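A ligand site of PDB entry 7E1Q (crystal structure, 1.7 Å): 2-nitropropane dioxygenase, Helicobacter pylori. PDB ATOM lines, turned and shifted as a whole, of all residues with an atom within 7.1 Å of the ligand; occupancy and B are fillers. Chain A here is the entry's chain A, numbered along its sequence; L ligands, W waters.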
ATOM      1  N   PHE A  83      30.991 -15.025  21.453  1.00  0.00           N
ATOM      2  CA  PHE A  83      30.177 -15.976  20.700  1.00  0.00           C
ATOM      3  C   PHE A  83      30.180 -15.649  19.216  1.00  0.00           C
ATOM      4  O   PHE A  83      30.247 -16.561  18.381  1.00  0.00           O
ATOM      5  CB  PHE A  83      28.743 -15.975  21.265  1.00  0.00           C
ATOM      6  CG  PHE A  83      27.856 -17.045  20.683  1.00  0.00           C
ATOM      7  CD1 PHE A  83      28.017 -18.384  21.004  1.00  0.00           C
ATOM      8  CD2 PHE A  83      26.862 -16.699  19.766  1.00  0.00           C
ATOM      9  CE1 PHE A  83      27.155 -19.356  20.454  1.00  0.00           C
ATOM     10  CE2 PHE A  83      26.018 -17.641  19.208  1.00  0.00           C
ATOM     11  CZ  PHE A  83      26.166 -18.985  19.554  1.00  0.00           C
ATOM     12  N   TYR A  84      30.059 -14.358  18.849  1.00  0.00           N
ATOM     13  CA  TYR A  84      30.208 -13.901  17.465  1.00  0.00           C
ATOM     14  C   TYR A  84      31.605 -13.284  17.366  1.00  0.00           C
ATOM     15  O   TYR A  84      31.781 -12.069  17.480  1.00  0.00           O
ATOM     16  CB  TYR A  84      29.120 -12.885  17.087  1.00  0.00           C
ATOM     17  CG  TYR A  84      27.730 -13.411  17.361  1.00  0.00           C
ATOM     18  CD1 TYR A  84      27.157 -14.387  16.543  1.00  0.00           C
ATOM     19  CD2 TYR A  84      27.010 -12.984  18.479  1.00  0.00           C
ATOM     20  CE1 TYR A  84      25.879 -14.886  16.814  1.00  0.00           C
ATOM     21  CE2 TYR A  84      25.735 -13.481  18.759  1.00  0.00           C
ATOM     22  CZ  TYR A  84      25.185 -14.436  17.933  1.00  0.00           C
ATOM     23  OH  TYR A  84      23.948 -14.950  18.205  1.00  0.00           O
ATOM     24  N   ASN A 114      21.919 -10.958  19.223  1.00  0.00           N
ATOM     25  CA  ASN A 114      22.547  -9.772  19.800  1.00  0.00           C
ATOM     26  C   ASN A 114      23.766  -9.377  18.973  1.00  0.00           C
ATOM     27  O   ASN A 114      24.409 -10.219  18.346  1.00  0.00           O
ATOM     28  CB  ASN A 114      22.935 -10.046  21.253  1.00  0.00           C
ATOM     29  CG  ASN A 114      21.739 -10.015  22.166  1.00  0.00           C
ATOM     30  OD1 ASN A 114      20.867  -9.166  22.010  1.00  0.00           O
ATOM     31  ND2 ASN A 114      21.677 -10.960  23.095  1.00  0.00           N
ATOM     32  N   PRO A 283      14.323 -20.771  21.904  1.00  0.00           N
ATOM     33  CA  PRO A 283      14.492 -19.460  22.572  1.00  0.00           C
ATOM     34  C   PRO A 283      14.571 -18.300  21.601  1.00  0.00           C
ATOM     35  O   PRO A 283      14.433 -17.147  22.029  1.00  0.00           O
ATOM     36  CB  PRO A 283      15.802 -19.612  23.356  1.00  0.00           C
ATOM     37  CG  PRO A 283      16.274 -21.011  23.159  1.00  0.00           C
ATOM     38  CD  PRO A 283      15.517 -21.620  22.034  1.00  0.00           C
ATOM     39  N   VAL A 284      14.810 -18.569  20.314  1.00  0.00           N
ATOM     40  CA  VAL A 284      14.760 -17.499  19.317  1.00  0.00           C
ATOM     41  C   VAL A 284      13.346 -16.976  19.091  1.00  0.00           C
ATOM     42  O   VAL A 284      13.177 -15.849  18.600  1.00  0.00           O
ATOM     43  CB  VAL A 284      15.385 -18.012  18.005  1.00  0.00           C
ATOM     44  CG1 VAL A 284      15.543 -16.873  17.004  1.00  0.00           C
ATOM     45  CG2 VAL A 284      16.756 -18.630  18.287  1.00  0.00           C
ATOM     46  N   ILE A 307      20.263 -24.447  32.931  1.00  0.00           N
ATOM     47  CA  ILE A 307      20.416 -23.332  31.987  1.00  0.00           C
ATOM     48  C   ILE A 307      21.092 -22.124  32.631  1.00  0.00           C
ATOM     49  O   ILE A 307      20.729 -21.704  33.746  1.00  0.00           O
ATOM     50  CB  ILE A 307      19.088 -22.958  31.306  1.00  0.00           C
ATOM     51  CG1 ILE A 307      18.815 -23.955  30.157  1.00  0.00           C
ATOM     52  CG2 ILE A 307      19.094 -21.491  30.797  1.00  0.00           C
ATOM     53  CD1 ILE A 307      17.400 -24.012  29.742  1.00  0.00           C
ATOM     54  N   ALA A 308      22.098 -21.561  31.937  1.00  0.00           N
ATOM     55  CA  ALA A 308      22.841 -20.412  32.435  1.00  0.00           C
ATOM     56  C   ALA A 308      23.331 -19.596  31.246  1.00  0.00           C
ATOM     57  O   ALA A 308      24.177 -20.065  30.484  1.00  0.00           O
ATOM     58  CB  ALA A 308      24.006 -20.858  33.316  1.00  0.00           C
ATOM     59  N   CYS A 309      22.815 -18.370  31.080  1.00  0.00           N
ATOM     60  CA  CYS A 309      23.118 -17.615  29.867  1.00  0.00           C
ATOM     61  C   CYS A 309      24.551 -17.080  29.936  1.00  0.00           C
ATOM     62  O   CYS A 309      24.822 -16.096  30.616  1.00  0.00           O
ATOM     63  CB  CYS A 309      22.135 -16.465  29.673  1.00  0.00           C
ATOM     64  SG  CYS A 309      22.459 -15.504  28.178  1.00  0.00           S
ATOM     65  N   VAL A 310      25.450 -17.712  29.190  1.00  0.00           N
ATOM     66  CA  VAL A 310      26.834 -17.264  29.137  1.00  0.00           C
ATOM     67  C   VAL A 310      27.126 -16.525  27.835  1.00  0.00           C
ATOM     68  O   VAL A 310      27.745 -15.454  27.854  1.00  0.00           O
ATOM     69  CB  VAL A 310      27.787 -18.461  29.314  1.00  0.00           C
ATOM     70  CG1 VAL A 310      29.233 -18.052  29.018  1.00  0.00           C
ATOM     71  CG2 VAL A 310      27.643 -19.080  30.706  1.00  0.00           C
ATOM     72  N   SER A 311      26.684 -17.072  26.709  1.00  0.00           N
ATOM     73  CA  SER A 311      27.020 -16.510  25.406  1.00  0.00           C
ATOM     74  C   SER A 311      26.103 -15.364  24.995  1.00  0.00           C
ATOM     75  O   SER A 311      26.458 -14.596  24.091  1.00  0.00           O
ATOM     76  CB  SER A 311      26.965 -17.608  24.335  1.00  0.00           C
ATOM     77  OG  SER A 311      27.992 -18.575  24.557  1.00  0.00           O
ATOM     78  N   ASN A 312      24.942 -15.220  25.645  1.00  0.00           N
ATOM     79  CA  ASN A 312      23.989 -14.155  25.328  1.00  0.00           C
ATOM     80  C   ASN A 312      23.745 -14.035  23.823  1.00  0.00           C
ATOM     81  O   ASN A 312      23.873 -12.963  23.226  1.00  0.00           O
ATOM     82  CB  ASN A 312      24.446 -12.815  25.902  1.00  0.00           C
ATOM     83  CG  ASN A 312      23.352 -11.779  25.878  1.00  0.00           C
ATOM     84  OD1 ASN A 312      22.171 -12.115  25.934  1.00  0.00           O
ATOM     85  ND2 ASN A 312      23.732 -10.517  25.741  1.00  0.00           N
ATOM     86  N   CYS A 313      23.319 -15.154  23.223  1.00  0.00           N
ATOM     87  CA  CYS A 313      23.358 -15.226  21.769  1.00  0.00           C
ATOM     88  C   CYS A 313      22.236 -14.433  21.093  1.00  0.00           C
ATOM     89  O   CYS A 313      22.489 -13.842  20.030  1.00  0.00           O
ATOM     90  CB  CYS A 313      23.329 -16.694  21.311  1.00  0.00           C
ATOM     91  SG  CYS A 313      21.822 -17.622  21.699  1.00  0.00           S
ATOM     92  N   VAL A 314      21.001 -14.421  21.623  1.00  0.00           N
ATOM     93  CA  VAL A 314      19.880 -13.846  20.870  1.00  0.00           C
ATOM     94  C   VAL A 314      19.040 -12.936  21.753  1.00  0.00           C
ATOM     95  O   VAL A 314      18.782 -13.234  22.917  1.00  0.00           O
ATOM     96  CB  VAL A 314      18.999 -14.925  20.192  1.00  0.00           C
ATOM     97  CG1 VAL A 314      19.769 -15.636  19.053  1.00  0.00           C
ATOM     98  CG2 VAL A 314      18.435 -15.937  21.207  1.00  0.00           C
ATOM     99  N   ALA A 315      18.584 -11.827  21.166  1.00  0.00           N
ATOM    100  CA  ALA A 315      17.744 -10.874  21.898  1.00  0.00           C
ATOM    101  C   ALA A 315      16.411 -11.440  22.359  1.00  0.00           C
ATOM    102  O   ALA A 315      15.988 -11.111  23.481  1.00  0.00           O
ATOM    103  CB  ALA A 315      17.533  -9.613  21.047  1.00  0.00           C
ATOM    104  N   PRO A 316      15.672 -12.227  21.565  1.00  0.00           N
ATOM    105  CA  PRO A 316      14.348 -12.691  22.053  1.00  0.00           C
ATOM    106  C   PRO A 316      14.403 -13.517  23.322  1.00  0.00           C
ATOM    107  O   PRO A 316      13.419 -13.569  24.072  1.00  0.00           O
ATOM    108  CB  PRO A 316      13.809 -13.500  20.871  1.00  0.00           C
ATOM    109  CG  PRO A 316      14.492 -12.883  19.654  1.00  0.00           C
ATOM    110  CD  PRO A 316      15.878 -12.554  20.137  1.00  0.00           C
ATOM    111  N   CYS A 317      15.532 -14.188  23.593  1.00  0.00           N
ATOM    112  CA  CYS A 317      15.609 -15.049  24.776  1.00  0.00           C
ATOM    113  C   CYS A 317      15.593 -14.245  26.071  1.00  0.00           C
ATOM    114  O   CYS A 317      15.177 -14.766  27.119  1.00  0.00           O
ATOM    115  CB  CYS A 317      16.854 -15.920  24.685  1.00  0.00           C
ATOM    116  SG  CYS A 317      17.110 -17.029  26.080  1.00  0.00           S
ATOM    117  N   ASN A 318      16.032 -12.990  26.034  1.00  0.00           N
ATOM    118  CA  ASN A 318      16.125 -12.160  27.242  1.00  0.00           C
ATOM    119  C   ASN A 318      17.021 -12.801  28.296  1.00  0.00           C
ATOM    120  O   ASN A 318      16.637 -13.002  29.452  1.00  0.00           O
ATOM    121  CB  ASN A 318      14.734 -11.866  27.812  1.00  0.00           C
ATOM    122  CG  ASN A 318      14.734 -10.760  28.834  1.00  0.00           C
ATOM    123  OD1 ASN A 318      15.637  -9.924  28.846  1.00  0.00           O
ATOM    124  ND2 ASN A 318      13.770 -10.791  29.743  1.00  0.00           N
ATOM    125  N   ARG A 319      18.240 -13.160  27.877  1.00  0.00           N
ATOM    126  CA  ARG A 319      19.301 -13.640  28.781  1.00  0.00           C
ATOM    127  C   ARG A 319      18.868 -14.858  29.607  1.00  0.00           C
ATOM    128  O   ARG A 319      19.215 -14.987  30.791  1.00  0.00           O
ATOM    129  CB  ARG A 319      19.780 -12.531  29.702  1.00  0.00           C
ATOM    130  CG  ARG A 319      20.541 -11.419  28.966  1.00  0.00           C
ATOM    131  CD  ARG A 319      21.423 -10.667  29.934  1.00  0.00           C
ATOM    132  NE  ARG A 319      22.555 -10.026  29.279  1.00  0.00           N
ATOM    133  CZ  ARG A 319      23.783 -10.533  29.241  1.00  0.00           C
ATOM    134  NH1 ARG A 319      24.757  -9.863  28.626  1.00  0.00           N
ATOM    135  NH2 ARG A 319      24.053 -11.703  29.803  1.00  0.00           N
ATOM    136  N   GLY A 320      18.142 -15.781  28.983  1.00  0.00           N
ATOM    137  CA  GLY A 320      17.805 -17.033  29.608  1.00  0.00           C
ATOM    138  C   GLY A 320      16.339 -17.210  29.912  1.00  0.00           C
ATOM    139  O   GLY A 320      15.908 -18.341  30.172  1.00  0.00           O
ATOM    140  N   GLU A 321      15.540 -16.142  29.855  1.00  0.00           N
ATOM    141  CA  GLU A 321      14.124 -16.275  30.160  1.00  0.00           C
ATOM    142  C   GLU A 321      13.448 -17.308  29.264  1.00  0.00           C
ATOM    143  O   GLU A 321      12.746 -18.208  29.738  1.00  0.00           O
ATOM    144  CB  GLU A 321      13.424 -14.923  30.019  1.00  0.00           C
ATOM    145  CG  GLU A 321      11.919 -15.063  30.256  1.00  0.00           C
ATOM    146  CD  GLU A 321      11.141 -13.800  29.970  1.00  0.00           C
ATOM    147  OE1 GLU A 321      11.761 -12.772  29.628  1.00  0.00           O
ATOM    148  OE2 GLU A 321       9.904 -13.866  30.081  1.00  0.00           O
ATOM    149  N   GLU A 322      13.653 -17.209  27.950  1.00  0.00           N
ATOM    150  CA  GLU A 322      12.949 -18.134  27.080  1.00  0.00           C
ATOM    151  C   GLU A 322      13.628 -19.495  27.040  1.00  0.00           C
ATOM    152  O   GLU A 322      12.948 -20.507  26.884  1.00  0.00           O
ATOM    153  CB  GLU A 322      12.843 -17.559  25.668  1.00  0.00           C
ATOM    154  CG  GLU A 322      12.063 -16.253  25.639  1.00  0.00           C
ATOM    155  CD  GLU A 322      10.635 -16.435  26.121  1.00  0.00           C
ATOM    156  OE1 GLU A 322      10.045 -17.517  25.865  1.00  0.00           O
ATOM    157  OE2 GLU A 322      10.112 -15.496  26.756  1.00  0.00           O
ATOM    158  N   ALA A 323      14.957 -19.531  27.177  1.00  0.00           N
ATOM    159  CA  ALA A 323      15.635 -20.817  27.232  1.00  0.00           C
ATOM    160  C   ALA A 323      15.107 -21.671  28.394  1.00  0.00           C
ATOM    161  O   ALA A 323      14.888 -22.872  28.238  1.00  0.00           O
ATOM    162  CB  ALA A 323      17.146 -20.630  27.353  1.00  0.00           C
ATOM    163  N   LYS A 324      14.906 -21.058  29.565  1.00  0.00           N
ATOM    164  CA  LYS A 324      14.368 -21.808  30.696  1.00  0.00           C
ATOM    165  C   LYS A 324      12.962 -22.310  30.407  1.00  0.00           C
ATOM    166  O   LYS A 324      12.595 -23.422  30.815  1.00  0.00           O
ATOM    167  CB  LYS A 324      14.392 -20.976  31.976  1.00  0.00           C
ATOM    168  CG  LYS A 324      15.783 -20.480  32.386  1.00  0.00           C
ATOM    169  CD  LYS A 324      15.725 -19.444  33.517  1.00  0.00           C
ATOM    170  CE  LYS A 324      17.044 -19.351  34.310  1.00  0.00           C
ATOM    171  NZ  LYS A 324      18.130 -18.556  33.648  1.00  0.00           N
ATOM    172  N   TYR A 328      16.069 -25.523  26.860  1.00  0.00           N
ATOM    173  CA  TYR A 328      17.436 -25.620  26.378  1.00  0.00           C
ATOM    174  C   TYR A 328      17.941 -24.260  25.922  1.00  0.00           C
ATOM    175  O   TYR A 328      17.164 -23.391  25.528  1.00  0.00           O
ATOM    176  CB  TYR A 328      17.560 -26.638  25.226  1.00  0.00           C
ATOM    177  CG  TYR A 328      16.891 -26.192  23.945  1.00  0.00           C
ATOM    178  CD1 TYR A 328      15.554 -26.500  23.707  1.00  0.00           C
ATOM    179  CD2 TYR A 328      17.600 -25.487  22.960  1.00  0.00           C
ATOM    180  CE1 TYR A 328      14.932 -26.098  22.544  1.00  0.00           C
ATOM    181  CE2 TYR A 328      16.968 -25.091  21.791  1.00  0.00           C
ATOM    182  CZ  TYR A 328      15.641 -25.393  21.590  1.00  0.00           C
ATOM    183  OH  TYR A 328      14.994 -25.003  20.436  1.00  0.00           O
ATOM    184  N   CYS A 329      19.265 -24.134  25.947  1.00  0.00           N
ATOM    185  CA  CYS A 329      19.990 -22.973  25.444  1.00  0.00           C
ATOM    186  C   CYS A 329      20.480 -23.284  24.030  1.00  0.00           C
ATOM    187  O   CYS A 329      21.189 -24.272  23.820  1.00  0.00           O
ATOM    188  CB  CYS A 329      21.167 -22.659  26.374  1.00  0.00           C
ATOM    189  SG  CYS A 329      22.362 -21.487  25.719  1.00  0.00           S
ATOM    190  N   ILE A 330      20.101 -22.458  23.060  1.00  0.00           N
ATOM    191  CA  ILE A 330      20.391 -22.835  21.678  1.00  0.00           C
ATOM    192  C   ILE A 330      21.878 -22.604  21.372  1.00  0.00           C
ATOM    193  O   ILE A 330      22.482 -23.356  20.608  1.00  0.00           O
ATOM    194  CB  ILE A 330      19.458 -22.101  20.706  1.00  0.00           C
ATOM    195  CG1 ILE A 330      19.528 -22.739  19.313  1.00  0.00           C
ATOM    196  CG2 ILE A 330      19.792 -20.598  20.646  1.00  0.00           C
ATOM    197  CD1 ILE A 330      18.531 -22.164  18.317  1.00  0.00           C
ATOM    198  N   ALA A 331      22.504 -21.595  21.982  1.00  0.00           N
ATOM    199  CA  ALA A 331      23.931 -21.391  21.801  1.00  0.00           C
ATOM    200  C   ALA A 331      24.727 -22.591  22.294  1.00  0.00           C
ATOM    201  O   ALA A 331      25.562 -23.141  21.566  1.00  0.00           O
ATOM    202  CB  ALA A 331      24.355 -20.131  22.551  1.00  0.00           C
ATOM    203  N   ASP A 332      24.468 -23.009  23.536  1.00  0.00           N
ATOM    204  CA  ASP A 332      25.179 -24.148  24.097  1.00  0.00           C
ATOM    205  C   ASP A 332      24.923 -25.410  23.301  1.00  0.00           C
ATOM    206  O   ASP A 332      25.848 -26.194  23.047  1.00  0.00           O
ATOM    207  CB  ASP A 332      24.742 -24.372  25.542  1.00  0.00           C
ATOM    208  CG  ASP A 332      25.152 -23.271  26.483  1.00  0.00           C
ATOM    209  OD1 ASP A 332      25.816 -22.289  26.072  1.00  0.00           O
ATOM    210  OD2 ASP A 332      24.788 -23.386  27.675  1.00  0.00           O
HETATM  211 FE1  LIG L   1      21.661 -16.909  26.526  1.00  0.00          FE
HETATM  212 FE2  LIG L   1      19.240 -17.706  25.677  1.00  0.00          FE
HETATM  213 FE3  LIG L   1      21.298 -19.476  25.702  1.00  0.00          FE
HETATM  214 FE4  LIG L   1      21.293 -17.556  23.907  1.00  0.00          FE
HETATM  215  S1  LIG L   1      19.673 -19.256  24.098  1.00  0.00           S
HETATM  216  S2  LIG L   1      23.107 -18.043  25.210  1.00  0.00           S
HETATM  217  S3  LIG L   1      20.356 -15.804  24.995  1.00  0.00           S
HETATM  218  S4  LIG L   1      20.356 -18.544  27.509  1.00  0.00           S
HETATM  219  O   HOH W   1      25.351 -19.694  27.018  1.00  0.00           O
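The backbone carbonyl oxygen (O) of Cys 313 is in hydrogen-bond range of the backbone NH (N) of Asn 114, 3.0 Å away. The backbone carbonyl oxygen (O) of Cys 313 is in hydrogen-bond range of the side-chain hydroxyl (OH) of Tyr 84, 2.6 Å away. The backbone NH (N) of Ala 331 sits close to the side-chain sulfur (SG) of Cys 329 (3.7 Å). The side-chain sulfur (SG) of Cys 329 sits close to the backbone NH (N) of Asp 332. N of Asn 312 lies close to SG of Cys 309 (3.6 Å). ND2 of Asn 312 lies close to NH1 of Arg 319, at 3.1 Å. The backbone carbonyl oxygen of Asn 312 sits at hydrogen-bond distance from the side-chain amide nitrogen of Asn 114. O of Ala 323 sits at hydrogen-bond distance from N of Tyr 328, at 3.2 Å.
SG of Cys 317 is bound to FE2 of the ligand (2.3 Å). S2 of the ligand lies close to N of Cys 313, at 3.5 Å. FE4 of the ligand is bound by SG of Cys 313, at 2.3 Å. FE3 of the ligand is bound by SG of Cys 329 (2.3 Å). The side-chain sulfur of Cys 309 binds an iron atom (FE1) of the ligand (2.3 Å). The backbone NH (N) of Ile 330 lies close to a sulfur (S1) of the ligand. N of Asn 312 sits close to S2 of the ligand (3.4 Å). The backbone NH (N) of Val 314 lies close to a sulfur (S3) of the ligand, at 3.7 Å.
Water W1 lies within hydrogen-bond range of OD1 of Asp 332, N of Val 310, N of Ser 311 and S2 of the ligand.
CG of Pro 283 touches S1 of the ligand (3.9 Å). CB of Ser 311 touches S2 of the ligand, 3.98 Å away. Gly 320 touches the ligand. CB of Ala 323 touches S4 of the ligand, 3.8 Å away. Ala 331 touches the ligand. Hydrophobic or aromatic side chains within 4 Å of the ligand: Pro 283, Ala 323, Ile 330 and Ala 331. 12 residues have an atom within 4 Å of the ligand: Pro 283, Cys 309, Ser 311, Asn 312, Cys 313, Val 314, Cys 317, Gly 320, Ala 323, Cys 329, Ile 330 and Ala 331. Along chain A the residues within 4 Å of the ligand span positions 283 to 331.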
